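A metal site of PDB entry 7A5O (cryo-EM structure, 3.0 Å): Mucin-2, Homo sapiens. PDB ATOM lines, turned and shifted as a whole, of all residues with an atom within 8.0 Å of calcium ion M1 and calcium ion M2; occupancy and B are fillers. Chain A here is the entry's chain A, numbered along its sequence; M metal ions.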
ATOM      1  N   ILE A1289      -0.733 -35.905  11.856  1.00  0.00           N
ATOM      2  CA  ILE A1289      -0.304 -34.841  10.953  1.00  0.00           C
ATOM      3  C   ILE A1289       0.303 -33.738  11.803  1.00  0.00           C
ATOM      4  O   ILE A1289      -0.422 -33.011  12.500  1.00  0.00           O
ATOM      5  CB  ILE A1289      -1.477 -34.301  10.107  1.00  0.00           C
ATOM      6  CG1 ILE A1289      -2.046 -35.420   9.245  1.00  0.00           C
ATOM      7  CG2 ILE A1289      -1.010 -33.169   9.228  1.00  0.00           C
ATOM      8  CD1 ILE A1289      -3.360 -35.066   8.587  1.00  0.00           C
ATOM      9  N   ASN A1290       1.624 -33.615  11.752  1.00  0.00           N
ATOM     10  CA  ASN A1290       2.353 -32.528  12.406  1.00  0.00           C
ATOM     11  C   ASN A1290       3.044 -31.753  11.290  1.00  0.00           C
ATOM     12  O   ASN A1290       4.203 -31.998  10.969  1.00  0.00           O
ATOM     13  CB  ASN A1290       3.356 -33.052  13.428  1.00  0.00           C
ATOM     14  CG  ASN A1290       3.899 -31.967  14.327  1.00  0.00           C
ATOM     15  OD1 ASN A1290       3.463 -30.818  14.283  1.00  0.00           O
ATOM     16  ND2 ASN A1290       4.905 -32.310  15.116  1.00  0.00           N
ATOM     17  N   GLU A1291       2.319 -30.809  10.695  1.00  0.00           N
ATOM     18  CA  GLU A1291       2.821 -30.060   9.555  1.00  0.00           C
ATOM     19  C   GLU A1291       3.052 -28.591   9.877  1.00  0.00           C
ATOM     20  O   GLU A1291       3.155 -27.762   8.964  1.00  0.00           O
ATOM     21  CB  GLU A1291       1.867 -30.195   8.366  1.00  0.00           C
ATOM     22  N   ASP A1292       3.128 -28.247  11.163  1.00  0.00           N
ATOM     23  CA  ASP A1292       3.326 -26.864  11.575  1.00  0.00           C
ATOM     24  C   ASP A1292       3.989 -26.885  12.946  1.00  0.00           C
ATOM     25  O   ASP A1292       3.951 -27.886  13.655  1.00  0.00           O
ATOM     26  CB  ASP A1292       1.983 -26.114  11.592  1.00  0.00           C
ATOM     27  CG  ASP A1292       2.143 -24.616  11.664  1.00  0.00           C
ATOM     28  OD1 ASP A1292       3.290 -24.122  11.714  1.00  0.00           O
ATOM     29  OD2 ASP A1292       1.113 -23.909  11.658  1.00  0.00           O
ATOM     30  N   HIS A1293       4.615 -25.769  13.300  1.00  0.00           N
ATOM     31  CA  HIS A1293       5.374 -25.672  14.537  1.00  0.00           C
ATOM     32  C   HIS A1293       5.176 -24.286  15.137  1.00  0.00           C
ATOM     33  O   HIS A1293       4.850 -23.331  14.419  1.00  0.00           O
ATOM     34  CB  HIS A1293       6.868 -25.931  14.295  1.00  0.00           C
ATOM     35  CG  HIS A1293       7.165 -27.324  13.856  1.00  0.00           C
ATOM     36  ND1 HIS A1293       7.165 -28.385  14.733  1.00  0.00           N
ATOM     37  CD2 HIS A1293       7.421 -27.838  12.629  1.00  0.00           C
ATOM     38  CE1 HIS A1293       7.438 -29.498  14.067  1.00  0.00           C
ATOM     39  NE2 HIS A1293       7.597 -29.192  12.795  1.00  0.00           N
ATOM     40  N   PRO A1294       5.339 -24.152  16.452  1.00  0.00           N
ATOM     41  CA  PRO A1294       5.286 -22.797  17.046  1.00  0.00           C
ATOM     42  C   PRO A1294       6.533 -21.974  16.764  1.00  0.00           C
ATOM     43  O   PRO A1294       6.427 -20.759  16.580  1.00  0.00           O
ATOM     44  CB  PRO A1294       5.127 -23.091  18.545  1.00  0.00           C
ATOM     45  CG  PRO A1294       4.553 -24.452  18.600  1.00  0.00           C
ATOM     46  CD  PRO A1294       5.176 -25.195  17.472  1.00  0.00           C
ATOM     47  N   SER A1295       7.703 -22.597  16.738  1.00  0.00           N
ATOM     48  CA  SER A1295       8.958 -21.897  16.497  1.00  0.00           C
ATOM     49  C   SER A1295       9.336 -21.852  15.018  1.00  0.00           C
ATOM     50  O   SER A1295      10.516 -21.714  14.691  1.00  0.00           O
ATOM     51  CB  SER A1295      10.090 -22.554  17.302  1.00  0.00           C
ATOM     52  OG  SER A1295      11.328 -21.912  17.066  1.00  0.00           O
ATOM     53  N   SER A1296       8.351 -21.989  14.129  1.00  0.00           N
ATOM     54  CA  SER A1296       8.554 -21.860  12.692  1.00  0.00           C
ATOM     55  C   SER A1296       7.214 -21.486  12.073  1.00  0.00           C
ATOM     56  O   SER A1296       6.209 -21.336  12.765  1.00  0.00           O
ATOM     57  CB  SER A1296       9.110 -23.152  12.068  1.00  0.00           C
ATOM     58  OG  SER A1296      10.415 -23.419  12.537  1.00  0.00           O
ATOM     59  N   GLY A1297       7.202 -21.327  10.752  1.00  0.00           N
ATOM     60  CA  GLY A1297       6.016 -20.896  10.060  1.00  0.00           C
ATOM     61  C   GLY A1297       5.809 -19.390  10.156  1.00  0.00           C
ATOM     62  O   GLY A1297       6.684 -18.636  10.601  1.00  0.00           O
ATOM     63  N   SER A1298       4.622 -18.959   9.731  1.00  0.00           N
ATOM     64  CA  SER A1298       4.294 -17.542   9.776  1.00  0.00           C
ATOM     65  C   SER A1298       2.845 -17.282  10.176  1.00  0.00           C
ATOM     66  O   SER A1298       2.372 -16.135  10.024  1.00  0.00           O
ATOM     67  CB  SER A1298       4.586 -16.877   8.429  1.00  0.00           C
ATOM     68  OG  SER A1298       5.970 -16.924   8.137  1.00  0.00           O
ATOM     69  N   ASP A1299       2.114 -18.271  10.676  1.00  0.00           N
ATOM     70  CA  ASP A1299       0.733 -18.086  11.088  1.00  0.00           C
ATOM     71  C   ASP A1299       0.586 -17.706  12.554  1.00  0.00           C
ATOM     72  O   ASP A1299      -0.550 -17.696  13.061  1.00  0.00           O
ATOM     73  CB  ASP A1299      -0.086 -19.354  10.770  1.00  0.00           C
ATOM     74  CG  ASP A1299       0.485 -20.612  11.414  1.00  0.00           C
ATOM     75  OD1 ASP A1299       1.553 -20.547  12.043  1.00  0.00           O
ATOM     76  OD2 ASP A1299      -0.169 -21.672  11.291  1.00  0.00           O
ATOM     77  N   ASP A1300       1.704 -17.405  13.238  1.00  0.00           N
ATOM     78  CA  ASP A1300       1.755 -16.878  14.613  1.00  0.00           C
ATOM     79  C   ASP A1300       1.117 -17.856  15.601  1.00  0.00           C
ATOM     80  O   ASP A1300       0.318 -17.476  16.463  1.00  0.00           O
ATOM     81  CB  ASP A1300       1.109 -15.483  14.682  1.00  0.00           C
ATOM     82  CG  ASP A1300       1.487 -14.710  15.937  1.00  0.00           C
ATOM     83  OD1 ASP A1300       2.277 -15.230  16.750  1.00  0.00           O
ATOM     84  OD2 ASP A1300       0.991 -13.583  16.108  1.00  0.00           O
ATOM     85  N   GLY A1301       1.459 -19.132  15.481  1.00  0.00           N
ATOM     86  CA  GLY A1301       0.854 -20.147  16.324  1.00  0.00           C
ATOM     87  C   GLY A1301       1.026 -21.551  15.789  1.00  0.00           C
ATOM     88  O   GLY A1301       2.127 -21.933  15.405  1.00  0.00           O
ATOM     89  N   ASP A1302      -0.052 -22.318  15.750  1.00  0.00           N
ATOM     90  CA  ASP A1302       0.007 -23.690  15.270  1.00  0.00           C
ATOM     91  C   ASP A1302      -1.354 -24.052  14.693  1.00  0.00           C
ATOM     92  O   ASP A1302      -2.363 -23.995  15.397  1.00  0.00           O
ATOM     93  CB  ASP A1302       0.392 -24.653  16.400  1.00  0.00           C
ATOM     94  CG  ASP A1302       0.794 -26.022  15.903  1.00  0.00           C
ATOM     95  OD1 ASP A1302       0.780 -26.252  14.679  1.00  0.00           O
ATOM     96  OD2 ASP A1302       1.133 -26.866  16.734  1.00  0.00           O
ATOM     97  N   ARG A1303      -1.385 -24.401  13.405  1.00  0.00           N
ATOM     98  CA  ARG A1303      -2.628 -24.732  12.727  1.00  0.00           C
ATOM     99  C   ARG A1303      -2.422 -25.966  11.872  1.00  0.00           C
ATOM    100  O   ARG A1303      -1.503 -26.017  11.057  1.00  0.00           O
ATOM    101  CB  ARG A1303      -3.111 -23.562  11.855  1.00  0.00           C
ATOM    102  CG  ARG A1303      -3.594 -22.363  12.652  1.00  0.00           C
ATOM    103  CD  ARG A1303      -4.047 -21.215  11.778  1.00  0.00           C
ATOM    104  NE  ARG A1303      -4.467 -20.080  12.581  1.00  0.00           N
ATOM    105  CZ  ARG A1303      -4.869 -18.913  12.081  1.00  0.00           C
ATOM    106  NH1 ARG A1303      -4.905 -18.731  10.775  1.00  0.00           N
ATOM    107  NH2 ARG A1303      -5.240 -17.935  12.898  1.00  0.00           N
ATOM    108  N   GLU A1304      -3.282 -26.961  12.064  1.00  0.00           N
ATOM    109  CA  GLU A1304      -3.186 -28.252  11.393  1.00  0.00           C
ATOM    110  C   GLU A1304      -4.504 -28.530  10.685  1.00  0.00           C
ATOM    111  O   GLU A1304      -5.547 -28.651  11.330  1.00  0.00           O
ATOM    112  CB  GLU A1304      -2.866 -29.367  12.383  1.00  0.00           C
ATOM    113  CG  GLU A1304      -1.492 -29.270  13.014  1.00  0.00           C
ATOM    114  CD  GLU A1304      -0.388 -29.519  12.021  1.00  0.00           C
ATOM    115  OE1 GLU A1304      -0.586 -30.332  11.091  1.00  0.00           O
ATOM    116  OE2 GLU A1304       0.688 -28.903  12.154  1.00  0.00           O
ATOM    117  N   ARG A1319      -4.245 -33.836  19.957  1.00  0.00           N
ATOM    118  CA  ARG A1319      -3.250 -34.186  20.963  1.00  0.00           C
ATOM    119  C   ARG A1319      -1.965 -33.411  20.763  1.00  0.00           C
ATOM    120  O   ARG A1319      -1.819 -32.640  19.810  1.00  0.00           O
ATOM    121  CB  ARG A1319      -2.957 -35.699  20.964  1.00  0.00           C
ATOM    122  CG  ARG A1319      -4.145 -36.535  21.370  1.00  0.00           C
ATOM    123  CD  ARG A1319      -4.457 -36.262  22.820  1.00  0.00           C
ATOM    124  NE  ARG A1319      -5.631 -36.989  23.291  1.00  0.00           N
ATOM    125  CZ  ARG A1319      -5.598 -38.203  23.815  1.00  0.00           C
ATOM    126  NH1 ARG A1319      -4.442 -38.845  23.918  1.00  0.00           N
ATOM    127  NH2 ARG A1319      -6.713 -38.782  24.218  1.00  0.00           N
ATOM    128  N   SER A1320      -1.029 -33.596  21.690  1.00  0.00           N
ATOM    129  CA  SER A1320       0.252 -32.915  21.677  1.00  0.00           C
ATOM    130  C   SER A1320       1.368 -33.874  21.275  1.00  0.00           C
ATOM    131  O   SER A1320       1.235 -35.085  21.390  1.00  0.00           O
ATOM    132  CB  SER A1320       0.583 -32.307  23.035  1.00  0.00           C
ATOM    133  OG  SER A1320       1.847 -31.664  23.018  1.00  0.00           O
ATOM    134  N   VAL A1321       2.476 -33.293  20.821  1.00  0.00           N
ATOM    135  CA  VAL A1321       3.567 -34.100  20.290  1.00  0.00           C
ATOM    136  C   VAL A1321       4.376 -34.724  21.420  1.00  0.00           C
ATOM    137  O   VAL A1321       4.547 -35.938  21.481  1.00  0.00           O
ATOM    138  CB  VAL A1321       4.443 -33.248  19.362  1.00  0.00           C
ATOM    139  CG1 VAL A1321       5.643 -34.040  18.918  1.00  0.00           C
ATOM    140  CG2 VAL A1321       3.648 -32.802  18.194  1.00  0.00           C
ATOM    141  N   PHE A1343      -7.538 -27.302  13.276  1.00  0.00           N
ATOM    142  CA  PHE A1343      -6.961 -26.900  14.556  1.00  0.00           C
ATOM    143  C   PHE A1343      -6.423 -25.486  14.440  1.00  0.00           C
ATOM    144  O   PHE A1343      -5.805 -25.139  13.430  1.00  0.00           O
ATOM    145  CB  PHE A1343      -5.849 -27.862  14.977  1.00  0.00           C
ATOM    146  CG  PHE A1343      -5.224 -27.524  16.291  1.00  0.00           C
ATOM    147  CD1 PHE A1343      -5.886 -27.769  17.474  1.00  0.00           C
ATOM    148  CD2 PHE A1343      -3.967 -26.948  16.344  1.00  0.00           C
ATOM    149  CE1 PHE A1343      -5.321 -27.447  18.677  1.00  0.00           C
ATOM    150  CE2 PHE A1343      -3.394 -26.629  17.552  1.00  0.00           C
ATOM    151  CZ  PHE A1343      -4.078 -26.871  18.712  1.00  0.00           C
ATOM    152  N   CYS A1345      -4.360 -22.592  16.936  1.00  0.00           N
ATOM    153  CA  CYS A1345      -3.756 -22.013  18.134  1.00  0.00           C
ATOM    154  C   CYS A1345      -3.123 -20.694  17.726  1.00  0.00           C
ATOM    155  O   CYS A1345      -2.420 -20.629  16.714  1.00  0.00           O
ATOM    156  CB  CYS A1345      -2.712 -22.954  18.761  1.00  0.00           C
ATOM    157  SG  CYS A1345      -2.009 -22.432  20.360  1.00  0.00           S
ATOM    158  N   ASN A1347      -0.782 -17.416  19.132  1.00  0.00           N
ATOM    159  CA  ASN A1347       0.141 -17.026  20.206  1.00  0.00           C
ATOM    160  C   ASN A1347      -0.352 -15.817  20.983  1.00  0.00           C
ATOM    161  O   ASN A1347       0.046 -15.633  22.135  1.00  0.00           O
ATOM    162  CB  ASN A1347       1.535 -16.713  19.658  1.00  0.00           C
ATOM    163  CG  ASN A1347       2.306 -17.949  19.265  1.00  0.00           C
ATOM    164  OD1 ASN A1347       2.246 -18.960  19.946  1.00  0.00           O
ATOM    165  ND2 ASN A1347       3.055 -17.853  18.180  1.00  0.00           N
ATOM    166  N   TYR A1360       1.946 -24.820  22.291  1.00  0.00           N
ATOM    167  CA  TYR A1360       2.646 -26.095  22.348  1.00  0.00           C
ATOM    168  C   TYR A1360       2.608 -26.708  20.954  1.00  0.00           C
ATOM    169  O   TYR A1360       2.005 -26.173  20.029  1.00  0.00           O
ATOM    170  CB  TYR A1360       2.012 -26.991  23.409  1.00  0.00           C
ATOM    171  CG  TYR A1360       2.144 -26.472  24.822  1.00  0.00           C
ATOM    172  CD1 TYR A1360       3.155 -25.581  25.177  1.00  0.00           C
ATOM    173  CD2 TYR A1360       1.200 -26.790  25.785  1.00  0.00           C
ATOM    174  CE1 TYR A1360       3.237 -25.090  26.453  1.00  0.00           C
ATOM    175  CE2 TYR A1360       1.285 -26.289  27.059  1.00  0.00           C
ATOM    176  CZ  TYR A1360       2.302 -25.439  27.386  1.00  0.00           C
ATOM    177  OH  TYR A1360       2.406 -24.926  28.651  1.00  0.00           O
ATOM    178  N   ASP A1361       3.261 -27.846  20.785  1.00  0.00           N
ATOM    179  CA  ASP A1361       3.352 -28.494  19.484  1.00  0.00           C
ATOM    180  C   ASP A1361       2.281 -29.574  19.423  1.00  0.00           C
ATOM    181  O   ASP A1361       2.307 -30.512  20.215  1.00  0.00           O
ATOM    182  CB  ASP A1361       4.743 -29.067  19.277  1.00  0.00           C
ATOM    183  CG  ASP A1361       5.007 -29.460  17.844  1.00  0.00           C
ATOM    184  OD1 ASP A1361       4.123 -29.299  16.983  1.00  0.00           O
ATOM    185  OD2 ASP A1361       6.135 -29.922  17.573  1.00  0.00           O
ATOM    186  N   TYR A1362       1.348 -29.422  18.499  1.00  0.00           N
ATOM    187  CA  TYR A1362       0.161 -30.271  18.411  1.00  0.00           C
ATOM    188  C   TYR A1362       0.193 -31.109  17.137  1.00  0.00           C
ATOM    189  O   TYR A1362       0.972 -30.864  16.214  1.00  0.00           O
ATOM    190  CB  TYR A1362      -1.095 -29.408  18.443  1.00  0.00           C
ATOM    191  CG  TYR A1362      -1.390 -28.746  19.768  1.00  0.00           C
ATOM    192  CD1 TYR A1362      -2.104 -29.402  20.757  1.00  0.00           C
ATOM    193  CD2 TYR A1362      -0.942 -27.456  20.034  1.00  0.00           C
ATOM    194  CE1 TYR A1362      -2.380 -28.802  21.951  1.00  0.00           C
ATOM    195  CE2 TYR A1362      -1.210 -26.845  21.240  1.00  0.00           C
ATOM    196  CZ  TYR A1362      -1.929 -27.520  22.187  1.00  0.00           C
ATOM    197  OH  TYR A1362      -2.197 -26.921  23.386  1.00  0.00           O
ATOM    198  N   LYS A1363      -0.680 -32.111  17.107  1.00  0.00           N
ATOM    199  CA  LYS A1363      -0.820 -33.027  15.976  1.00  0.00           C
ATOM    200  C   LYS A1363      -2.225 -33.586  15.992  1.00  0.00           C
ATOM    201  O   LYS A1363      -2.874 -33.629  17.042  1.00  0.00           O
ATOM    202  CB  LYS A1363       0.229 -34.132  16.033  1.00  0.00           C
ATOM    203  CG  LYS A1363       0.087 -35.054  17.222  1.00  0.00           C
ATOM    204  CD  LYS A1363       1.171 -36.100  17.260  1.00  0.00           C
ATOM    205  CE  LYS A1363       0.991 -37.010  18.439  1.00  0.00           C
ATOM    206  NZ  LYS A1363       2.051 -38.046  18.485  1.00  0.00           N
ATOM    207  N   ILE A1364      -2.732 -33.986  14.822  1.00  0.00           N
ATOM    208  CA  ILE A1364      -4.129 -34.412  14.684  1.00  0.00           C
ATOM    209  C   ILE A1364      -4.269 -35.671  13.842  1.00  0.00           C
ATOM    210  O   ILE A1364      -3.432 -35.995  12.997  1.00  0.00           O
ATOM    211  CB  ILE A1364      -5.039 -33.308  14.072  1.00  0.00           C
ATOM    212  CG1 ILE A1364      -4.556 -32.920  12.676  1.00  0.00           C
ATOM    213  CG2 ILE A1364      -5.188 -32.109  15.001  1.00  0.00           C
ATOM    214  CD1 ILE A1364      -5.538 -32.054  11.920  1.00  0.00           C
HETATM  215 CA    CA M   1       3.694 -21.768  12.649  1.00  0.00          CA
HETATM  216 CA    CA M   2       2.124 -28.829  15.174  1.00  0.00          CA
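The backbone NH (N) of Asp 1292 sits at hydrogen-bond distance from the side-chain carboxylate (OE2) of Glu 1304 (2.7 Å).
OD2 of Asp 1292 is in hydrogen-bond range of N of Arg 1303 (3.1 Å).
A ring nitrogen (ND1) of His 1293 is in hydrogen-bond range of the side-chain carboxylate (OD2) of Asp 1361 (3.4 Å).
O of Asp 1302 sits at hydrogen-bond distance from N of Cys 1345, at 2.9 Å.
O of Asp 1361 sits at hydrogen-bond distance from OG of Ser 1320 (3.1 Å).
ND2 of Asn 1347 lies close to N of Gly 1301 (3.4 Å).
The backbone NH (N) of Glu 1291 is in hydrogen-bond range of the side-chain carboxylate (OE2) of Glu 1304 (2.9 Å).
The backbone carbonyl oxygen (O) of Glu 1304 sits at hydrogen-bond distance from the backbone NH (N) of Phe 1343, at 3.1 Å.
Gly 1297 touches calcium ion M1 (CA to CA, 3.6 Å).
Gly 1301 touches calcium ion M1.
Residues that only touch calcium ion M2: Glu 1304 (3.3 Å).
Within 4 Å of calcium ion M2: Asn 1290, Asp 1292, Asp 1302, Glu 1304, Asp 1361 and Tyr 1362.
Along chain A the residues within 4 Å of calcium ion M2 span positions 1290 to 1362.
The nearest printed residue that does not touch calcium ion M2 is His 1293 (4.4 Å).
Calcium ion M1 is bound by the side-chain carboxylate (OD1) of Asp 1299 (2.5 Å), the backbone carbonyl oxygen (O) of Ser 1296 (2.6 Å), the side-chain carboxylate (OD1) of Asp 1292 (2.6 Å) and the backbone carbonyl oxygen (O) of His 1293 (2.6 Å).
Calcium ion M1 has four donor atoms within binding distance.
Calcium ion M2 is bound by the backbone carbonyl oxygen (O) of Asp 1292 (2.6 Å), the side-chain amide oxygen (OD1) of Asn 1290 (2.6 Å), the backbone carbonyl oxygen (O) of Tyr 1362 (2.6 Å), the side-chain carboxylate (OD2) of Asp 1302 (2.7 Å) and the side-chain carboxylate (OD1) of Asp 1361 (2.7 Å).
Slightly farther from calcium ion M2 lies the side-chain carboxylate (OD1) of Asp 1302 (2.9 Å).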
